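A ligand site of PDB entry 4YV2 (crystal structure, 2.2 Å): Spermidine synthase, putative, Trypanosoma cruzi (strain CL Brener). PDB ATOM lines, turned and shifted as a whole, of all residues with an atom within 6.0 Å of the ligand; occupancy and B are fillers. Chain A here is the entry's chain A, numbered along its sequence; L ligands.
O2 of the ligand sits at hydrogen-bond distance from OD1 of Asp 126 (2.8 Å).
NE2 of His 82 is in hydrogen-bond range of N1 of the ligand (2.8 Å).
O2 of the ligand sits at hydrogen-bond distance from NE2 of Gln 48.
A nitrogen (N1) of the ligand is in salt-bridge range of the side-chain carboxylate (OD2) of Asp 106.
The backbone NH of Gly 158 is in hydrogen-bond range of a nitrogen (N6) of the ligand (2.9 Å).
A sulfur (S1) of the ligand lies close to the backbone carbonyl oxygen (O) of Asp 176, 3.7 Å away.
OD2 of Asp 176 lies within salt-bridge range of N1 of the ligand (3.2 Å).
The side-chain carboxylate (OD1) of Asp 157 sits at hydrogen-bond distance from a nitrogen (N4) of the ligand.
N5 of the ligand lies within hydrogen-bond range of N of Ile 127 (3.3 Å).
O of Asp 126 sits at hydrogen-bond distance from N of Gly 156 (3.3 Å).
The backbone NH of Gly 104 sits at hydrogen-bond distance from the side-chain carboxylate of Asp 126, at 3.4 Å.
The side-chain carboxylate (OD1) of Asp 106 is in hydrogen-bond range of a ring nitrogen (NE2) of His 82 (3.4 Å).
The side-chain amide nitrogen of Gln 48 sits at hydrogen-bond distance from the side-chain carboxylate of Asp 128 (3.3 Å).
The backbone NH (N) of Gly 108 is in hydrogen-bond range of the side-chain carboxylate (OD1) of Asp 106, at 2.8 Å.
The side-chain carboxylate of Asp 176 lies within hydrogen-bond range of the side-chain hydroxyl of Tyr 81 (3.0 Å).
The backbone NH (N) of Gln 72 lies within hydrogen-bond range of the backbone carbonyl oxygen (O) of Met 65, 2.6 Å away.
N of Gly 103 is in hydrogen-bond range of O of Val 125, at 2.8 Å.
Merely in contact with the ligand: Gln 72 (3.1 Å), Val 131 (3.3 Å), Thr 177 (3.4 Å), Asp 128 (3.5 Å), Gly 103 (3.5 Å), Tyr 81 (3.6 Å), Val 125 (3.7 Å), Leu 67 (3.7 Å), Gly 156 (3.8 Å) and Tyr 245 (3.9 Å).
Hydrophobic or aromatic side chains within 4 Å of the ligand: Leu 67, Tyr 81, His 82, Ile 127 and Val 131.
Of the 26 residues printed, 18 come within 4 Å of the ligand.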
ATOM      1  N   GLN A  48     -18.547 -17.206 -12.342  1.00  0.00           N
ATOM      2  CA  GLN A  48     -19.886 -16.674 -12.336  1.00  0.00           C
ATOM      3  C   GLN A  48     -19.832 -15.196 -12.766  1.00  0.00           C
ATOM      4  O   GLN A  48     -18.750 -14.615 -12.813  1.00  0.00           O
ATOM      5  CB  GLN A  48     -20.555 -16.911 -10.936  1.00  0.00           C
ATOM      6  CG  GLN A  48     -19.797 -16.319  -9.751  1.00  0.00           C
ATOM      7  CD  GLN A  48     -19.947 -17.047  -8.403  1.00  0.00           C
ATOM      8  OE1 GLN A  48     -21.032 -17.476  -8.037  1.00  0.00           O
ATOM      9  NE2 GLN A  48     -18.858 -17.137  -7.648  1.00  0.00           N
ATOM     10  N   MET A  65     -24.196  -6.948  -3.540  1.00  0.00           N
ATOM     11  CA  MET A  65     -23.504  -7.903  -4.383  1.00  0.00           C
ATOM     12  C   MET A  65     -24.462  -8.915  -4.993  1.00  0.00           C
ATOM     13  O   MET A  65     -25.253  -9.568  -4.266  1.00  0.00           O
ATOM     14  CB  MET A  65     -22.444  -8.674  -3.611  1.00  0.00           C
ATOM     15  CG  MET A  65     -21.681  -9.695  -4.449  1.00  0.00           C
ATOM     16  SD  MET A  65     -20.620 -10.813  -3.527  1.00  0.00           S
ATOM     17  CE  MET A  65     -19.429  -9.694  -2.800  1.00  0.00           C
ATOM     18  N   LEU A  67     -24.630 -12.424  -7.641  1.00  0.00           N
ATOM     19  CA  LEU A  67     -23.885 -13.453  -8.338  1.00  0.00           C
ATOM     20  C   LEU A  67     -24.839 -14.137  -9.274  1.00  0.00           C
ATOM     21  O   LEU A  67     -25.875 -14.625  -8.864  1.00  0.00           O
ATOM     22  CB  LEU A  67     -23.231 -14.445  -7.344  1.00  0.00           C
ATOM     23  CG  LEU A  67     -22.035 -13.917  -6.514  1.00  0.00           C
ATOM     24  CD1 LEU A  67     -21.658 -14.869  -5.392  1.00  0.00           C
ATOM     25  CD2 LEU A  67     -20.794 -13.684  -7.334  1.00  0.00           C
ATOM     26  N   GLN A  72     -26.836 -11.318  -3.098  1.00  0.00           N
ATOM     27  CA  GLN A  72     -26.279 -12.255  -2.173  1.00  0.00           C
ATOM     28  C   GLN A  72     -25.911 -11.568  -0.902  1.00  0.00           C
ATOM     29  O   GLN A  72     -25.998 -12.190   0.177  1.00  0.00           O
ATOM     30  CB  GLN A  72     -25.054 -12.936  -2.788  1.00  0.00           C
ATOM     31  CG  GLN A  72     -25.331 -13.773  -4.044  1.00  0.00           C
ATOM     32  CD  GLN A  72     -25.788 -15.196  -3.751  1.00  0.00           C
ATOM     33  OE1 GLN A  72     -25.487 -15.747  -2.685  1.00  0.00           O
ATOM     34  NE2 GLN A  72     -26.511 -15.792  -4.697  1.00  0.00           N
ATOM     35  N   VAL A  73     -25.489 -10.298  -1.001  1.00  0.00           N
ATOM     36  CA  VAL A  73     -25.085  -9.540   0.179  1.00  0.00           C
ATOM     37  C   VAL A  73     -25.491  -8.075  -0.008  1.00  0.00           C
ATOM     38  O   VAL A  73     -25.255  -7.503  -1.041  1.00  0.00           O
ATOM     39  CB  VAL A  73     -23.548  -9.577   0.418  1.00  0.00           C
ATOM     40  CG1 VAL A  73     -23.211  -9.007   1.781  1.00  0.00           C
ATOM     41  CG2 VAL A  73     -22.982 -10.976   0.279  1.00  0.00           C
ATOM     42  N   TYR A  81     -27.784 -13.329   8.337  1.00  0.00           N
ATOM     43  CA  TYR A  81     -27.304 -14.608   7.816  1.00  0.00           C
ATOM     44  C   TYR A  81     -25.888 -14.979   8.327  1.00  0.00           C
ATOM     45  O   TYR A  81     -25.601 -16.135   8.548  1.00  0.00           O
ATOM     46  CB  TYR A  81     -27.288 -14.522   6.285  1.00  0.00           C
ATOM     47  CG  TYR A  81     -26.794 -15.771   5.602  1.00  0.00           C
ATOM     48  CD1 TYR A  81     -27.684 -16.806   5.287  1.00  0.00           C
ATOM     49  CD2 TYR A  81     -25.460 -15.948   5.259  1.00  0.00           C
ATOM     50  CE1 TYR A  81     -27.263 -17.971   4.657  1.00  0.00           C
ATOM     51  CE2 TYR A  81     -25.039 -17.113   4.629  1.00  0.00           C
ATOM     52  CZ  TYR A  81     -25.960 -18.099   4.335  1.00  0.00           C
ATOM     53  OH  TYR A  81     -25.609 -19.247   3.709  1.00  0.00           O
ATOM     54  N   HIS A  82     -24.985 -13.990   8.475  1.00  0.00           N
ATOM     55  CA  HIS A  82     -23.612 -14.254   8.885  1.00  0.00           C
ATOM     56  C   HIS A  82     -23.512 -14.589  10.350  1.00  0.00           C
ATOM     57  O   HIS A  82     -22.706 -15.415  10.756  1.00  0.00           O
ATOM     58  CB  HIS A  82     -22.719 -13.061   8.545  1.00  0.00           C
ATOM     59  CG  HIS A  82     -22.551 -12.868   7.080  1.00  0.00           C
ATOM     60  ND1 HIS A  82     -22.560 -11.632   6.471  1.00  0.00           N
ATOM     61  CD2 HIS A  82     -22.439 -13.785   6.088  1.00  0.00           C
ATOM     62  CE1 HIS A  82     -22.433 -11.799   5.172  1.00  0.00           C
ATOM     63  NE2 HIS A  82     -22.337 -13.088   4.916  1.00  0.00           N
ATOM     64  N   ILE A 102     -16.716 -23.262   3.815  1.00  0.00           N
ATOM     65  CA  ILE A 102     -16.711 -23.467   2.366  1.00  0.00           C
ATOM     66  C   ILE A 102     -17.604 -22.388   1.747  1.00  0.00           C
ATOM     67  O   ILE A 102     -18.708 -22.177   2.243  1.00  0.00           O
ATOM     68  CB  ILE A 102     -17.239 -24.883   2.063  1.00  0.00           C
ATOM     69  CG1 ILE A 102     -16.246 -25.921   2.591  1.00  0.00           C
ATOM     70  CG2 ILE A 102     -17.489 -25.031   0.581  1.00  0.00           C
ATOM     71  CD1 ILE A 102     -16.821 -27.330   2.743  1.00  0.00           C
ATOM     72  N   GLY A 103     -17.166 -21.697   0.692  1.00  0.00           N
ATOM     73  CA  GLY A 103     -17.868 -20.494   0.188  1.00  0.00           C
ATOM     74  C   GLY A 103     -17.479 -19.347   1.130  1.00  0.00           C
ATOM     75  O   GLY A 103     -16.374 -19.348   1.640  1.00  0.00           O
ATOM     76  N   GLY A 104     -18.377 -18.395   1.386  1.00  0.00           N
ATOM     77  CA  GLY A 104     -18.080 -17.338   2.355  1.00  0.00           C
ATOM     78  C   GLY A 104     -16.943 -16.404   1.938  1.00  0.00           C
ATOM     79  O   GLY A 104     -16.330 -15.723   2.777  1.00  0.00           O
ATOM     80  N   GLY A 105     -16.715 -16.336   0.632  1.00  0.00           N
ATOM     81  CA  GLY A 105     -15.697 -15.480   0.054  1.00  0.00           C
ATOM     82  C   GLY A 105     -15.725 -14.017   0.494  1.00  0.00           C
ATOM     83  O   GLY A 105     -14.668 -13.351   0.484  1.00  0.00           O
ATOM     84  N   ASP A 106     -16.918 -13.523   0.879  1.00  0.00           N
ATOM     85  CA  ASP A 106     -17.066 -12.108   1.260  1.00  0.00           C
ATOM     86  C   ASP A 106     -16.472 -11.824   2.626  1.00  0.00           C
ATOM     87  O   ASP A 106     -16.264 -10.657   2.996  1.00  0.00           O
ATOM     88  CB  ASP A 106     -18.544 -11.719   1.276  1.00  0.00           C
ATOM     89  CG  ASP A 106     -19.396 -12.722   2.010  1.00  0.00           C
ATOM     90  OD1 ASP A 106     -19.337 -12.722   3.262  1.00  0.00           O
ATOM     91  OD2 ASP A 106     -20.122 -13.504   1.323  1.00  0.00           O
ATOM     92  N   GLY A 108     -17.883 -12.516   5.632  1.00  0.00           N
ATOM     93  CA  GLY A 108     -18.923 -12.351   6.690  1.00  0.00           C
ATOM     94  C   GLY A 108     -19.052 -13.470   7.751  1.00  0.00           C
ATOM     95  O   GLY A 108     -19.026 -13.191   8.960  1.00  0.00           O
ATOM     96  N   VAL A 109     -19.222 -14.717   7.328  1.00  0.00           N
ATOM     97  CA  VAL A 109     -19.234 -15.797   8.348  1.00  0.00           C
ATOM     98  C   VAL A 109     -17.959 -15.825   9.206  1.00  0.00           C
ATOM     99  O   VAL A 109     -18.010 -16.001  10.439  1.00  0.00           O
ATOM    100  CB  VAL A 109     -19.454 -17.185   7.715  1.00  0.00           C
ATOM    101  CG1 VAL A 109     -19.360 -18.257   8.809  1.00  0.00           C
ATOM    102  CG2 VAL A 109     -20.833 -17.187   7.042  1.00  0.00           C
ATOM    103  N   VAL A 125     -12.353 -21.842   2.218  1.00  0.00           N
ATOM    104  CA  VAL A 125     -12.118 -22.046   0.804  1.00  0.00           C
ATOM    105  C   VAL A 125     -13.297 -21.518  -0.059  1.00  0.00           C
ATOM    106  O   VAL A 125     -14.429 -21.968   0.052  1.00  0.00           O
ATOM    107  CB  VAL A 125     -11.930 -23.568   0.547  1.00  0.00           C
ATOM    108  CG1 VAL A 125     -11.481 -23.849  -0.899  1.00  0.00           C
ATOM    109  CG2 VAL A 125     -10.930 -24.137   1.546  1.00  0.00           C
ATOM    110  N   ASP A 126     -13.023 -20.634  -0.986  1.00  0.00           N
ATOM    111  CA  ASP A 126     -14.040 -20.148  -1.896  1.00  0.00           C
ATOM    112  C   ASP A 126     -13.469 -20.228  -3.305  1.00  0.00           C
ATOM    113  O   ASP A 126     -12.360 -19.760  -3.545  1.00  0.00           O
ATOM    114  CB  ASP A 126     -14.442 -18.709  -1.573  1.00  0.00           C
ATOM    115  CG  ASP A 126     -15.732 -18.289  -2.271  1.00  0.00           C
ATOM    116  OD1 ASP A 126     -15.711 -18.245  -3.522  1.00  0.00           O
ATOM    117  OD2 ASP A 126     -16.761 -18.038  -1.569  1.00  0.00           O
ATOM    118  N   ILE A 127     -14.280 -20.718  -4.242  1.00  0.00           N
ATOM    119  CA  ILE A 127     -13.831 -21.087  -5.548  1.00  0.00           C
ATOM    120  C   ILE A 127     -13.483 -19.885  -6.366  1.00  0.00           C
ATOM    121  O   ILE A 127     -12.711 -19.983  -7.332  1.00  0.00           O
ATOM    122  CB  ILE A 127     -14.903 -21.959  -6.262  1.00  0.00           C
ATOM    123  CG1 ILE A 127     -14.306 -22.640  -7.529  1.00  0.00           C
ATOM    124  CG2 ILE A 127     -16.151 -21.138  -6.567  1.00  0.00           C
ATOM    125  CD1 ILE A 127     -15.106 -23.878  -7.979  1.00  0.00           C
ATOM    126  N   ASP A 128     -14.016 -18.725  -5.958  1.00  0.00           N
ATOM    127  CA  ASP A 128     -13.885 -17.512  -6.743  1.00  0.00           C
ATOM    128  C   ASP A 128     -13.101 -16.458  -5.990  1.00  0.00           C
ATOM    129  O   ASP A 128     -13.576 -15.836  -5.033  1.00  0.00           O
ATOM    130  CB  ASP A 128     -15.279 -16.982  -7.125  1.00  0.00           C
ATOM    131  CG  ASP A 128     -15.241 -15.969  -8.270  1.00  0.00           C
ATOM    132  OD1 ASP A 128     -14.294 -15.173  -8.318  1.00  0.00           O
ATOM    133  OD2 ASP A 128     -16.175 -15.984  -9.101  1.00  0.00           O
ATOM    134  N   VAL A 131     -14.543 -12.724  -5.978  1.00  0.00           N
ATOM    135  CA  VAL A 131     -15.496 -12.459  -4.894  1.00  0.00           C
ATOM    136  C   VAL A 131     -14.755 -11.924  -3.677  1.00  0.00           C
ATOM    137  O   VAL A 131     -15.166 -10.934  -3.077  1.00  0.00           O
ATOM    138  CB  VAL A 131     -16.285 -13.741  -4.558  1.00  0.00           C
ATOM    139  CG1 VAL A 131     -16.879 -13.666  -3.155  1.00  0.00           C
ATOM    140  CG2 VAL A 131     -17.344 -14.014  -5.636  1.00  0.00           C
ATOM    141  N   GLY A 156     -10.210 -22.165  -4.071  1.00  0.00           N
ATOM    142  CA  GLY A 156     -10.311 -23.586  -4.399  1.00  0.00           C
ATOM    143  C   GLY A 156     -11.738 -24.077  -4.363  1.00  0.00           C
ATOM    144  O   GLY A 156     -12.600 -23.496  -3.673  1.00  0.00           O
ATOM    145  N   ASP A 157     -12.000 -25.161  -5.089  1.00  0.00           N
ATOM    146  CA  ASP A 157     -13.271 -25.911  -5.014  1.00  0.00           C
ATOM    147  C   ASP A 157     -13.439 -26.532  -3.628  1.00  0.00           C
ATOM    148  O   ASP A 157     -12.593 -27.303  -3.209  1.00  0.00           O
ATOM    149  CB  ASP A 157     -13.311 -27.010  -6.100  1.00  0.00           C
ATOM    150  CG  ASP A 157     -14.651 -27.736  -6.177  1.00  0.00           C
ATOM    151  OD1 ASP A 157     -15.561 -27.443  -5.379  1.00  0.00           O
ATOM    152  OD2 ASP A 157     -14.794 -28.641  -7.034  1.00  0.00           O
ATOM    153  N   GLY A 158     -14.523 -26.222  -2.920  1.00  0.00           N
ATOM    154  CA  GLY A 158     -14.734 -26.782  -1.585  1.00  0.00           C
ATOM    155  C   GLY A 158     -14.871 -28.310  -1.649  1.00  0.00           C
ATOM    156  O   GLY A 158     -14.446 -29.047  -0.741  1.00  0.00           O
ATOM    157  N   LEU A 159     -15.459 -28.784  -2.750  1.00  0.00           N
ATOM    158  CA  LEU A 159     -15.605 -30.227  -2.922  1.00  0.00           C
ATOM    159  C   LEU A 159     -14.237 -30.935  -3.010  1.00  0.00           C
ATOM    160  O   LEU A 159     -14.024 -31.885  -2.281  1.00  0.00           O
ATOM    161  CB  LEU A 159     -16.449 -30.569  -4.147  1.00  0.00           C
ATOM    162  CG  LEU A 159     -16.747 -32.049  -4.320  1.00  0.00           C
ATOM    163  CD1 LEU A 159     -18.068 -32.436  -3.673  1.00  0.00           C
ATOM    164  CD2 LEU A 159     -16.767 -32.402  -5.804  1.00  0.00           C
ATOM    165  N   ASP A 176     -21.436 -22.086   3.128  1.00  0.00           N
ATOM    166  CA  ASP A 176     -22.065 -20.810   2.735  1.00  0.00           C
ATOM    167  C   ASP A 176     -21.867 -20.637   1.207  1.00  0.00           C
ATOM    168  O   ASP A 176     -21.168 -19.724   0.756  1.00  0.00           O
ATOM    169  CB  ASP A 176     -21.380 -19.686   3.530  1.00  0.00           C
ATOM    170  CG  ASP A 176     -21.901 -18.272   3.194  1.00  0.00           C
ATOM    171  OD1 ASP A 176     -22.999 -18.184   2.590  1.00  0.00           O
ATOM    172  OD2 ASP A 176     -21.221 -17.269   3.583  1.00  0.00           O
ATOM    173  N   THR A 177     -22.447 -21.554   0.439  1.00  0.00           N
ATOM    174  CA  THR A 177     -22.254 -21.597  -1.002  1.00  0.00           C
ATOM    175  C   THR A 177     -23.553 -21.273  -1.729  1.00  0.00           C
ATOM    176  O   THR A 177     -24.578 -21.927  -1.465  1.00  0.00           O
ATOM    177  CB  THR A 177     -21.832 -22.985  -1.462  1.00  0.00           C
ATOM    178  OG1 THR A 177     -22.884 -23.886  -1.138  1.00  0.00           O
ATOM    179  CG2 THR A 177     -20.571 -23.437  -0.759  1.00  0.00           C
ATOM    180  N   TYR A 245     -33.717 -11.382   0.666  1.00  0.00           N
ATOM    181  CA  TYR A 245     -33.709 -12.687  -0.036  1.00  0.00           C
ATOM    182  C   TYR A 245     -35.098 -13.029  -0.499  1.00  0.00           C
ATOM    183  O   TYR A 245     -36.037 -12.534   0.060  1.00  0.00           O
ATOM    184  CB  TYR A 245     -33.174 -13.811   0.842  1.00  0.00           C
ATOM    185  CG  TYR A 245     -31.663 -13.957   0.795  1.00  0.00           C
ATOM    186  CD1 TYR A 245     -30.824 -12.887   1.095  1.00  0.00           C
ATOM    187  CD2 TYR A 245     -31.069 -15.167   0.456  1.00  0.00           C
ATOM    188  CE1 TYR A 245     -29.429 -13.014   1.084  1.00  0.00           C
ATOM    189  CE2 TYR A 245     -29.675 -15.303   0.441  1.00  0.00           C
ATOM    190  CZ  TYR A 245     -28.875 -14.228   0.765  1.00  0.00           C
ATOM    191  OH  TYR A 245     -27.507 -14.378   0.764  1.00  0.00           O
HETATM  192  C1  LIG L   1     -23.639 -15.282   1.824  1.00  0.00           C
HETATM  193  N1  LIG L   1     -22.515 -14.559   2.537  1.00  0.00           N
HETATM  194  C2  LIG L   1     -23.707 -14.978   0.347  1.00  0.00           C
HETATM  195  C3  LIG L   1     -23.262 -16.154  -0.506  1.00  0.00           C
HETATM  196  S1  LIG L   1     -21.421 -16.342  -0.667  1.00  0.00           S
HETATM  197  C4  LIG L   1     -21.034 -14.864  -1.683  1.00  0.00           C
HETATM  198  C5  LIG L   1     -21.500 -17.679  -1.925  1.00  0.00           C
HETATM  199  C6  LIG L   1     -20.080 -18.124  -2.260  1.00  0.00           C
HETATM  200  O1  LIG L   1     -19.999 -19.536  -2.534  1.00  0.00           O
HETATM  201  C7  LIG L   1     -18.910 -19.687  -3.443  1.00  0.00           C
HETATM  202  C8  LIG L   1     -19.130 -18.542  -4.449  1.00  0.00           C
HETATM  203  O2  LIG L   1     -17.973 -18.146  -5.169  1.00  0.00           O
HETATM  204  C9  LIG L   1     -19.642 -17.433  -3.553  1.00  0.00           C
HETATM  205  O3  LIG L   1     -18.697 -16.460  -3.167  1.00  0.00           O
HETATM  206  N2  LIG L   1     -18.912 -21.028  -3.993  1.00  0.00           N
HETATM  207  C10 LIG L   1     -19.818 -21.521  -4.900  1.00  0.00           C
HETATM  208  N3  LIG L   1     -19.541 -22.783  -5.189  1.00  0.00           N
HETATM  209  C11 LIG L   1     -18.419 -23.116  -4.446  1.00  0.00           C
HETATM  210  C12 LIG L   1     -17.651 -24.261  -4.346  1.00  0.00           C
HETATM  211  N4  LIG L   1     -17.928 -25.403  -5.065  1.00  0.00           N
HETATM  212  C13 LIG L   1     -18.024 -22.036  -3.696  1.00  0.00           C
HETATM  213  N5  LIG L   1     -16.963 -22.031  -2.875  1.00  0.00           N
HETATM  214  C14 LIG L   1     -16.313 -23.191  -2.834  1.00  0.00           C
HETATM  215  N6  LIG L   1     -16.598 -24.302  -3.521  1.00  0.00           N
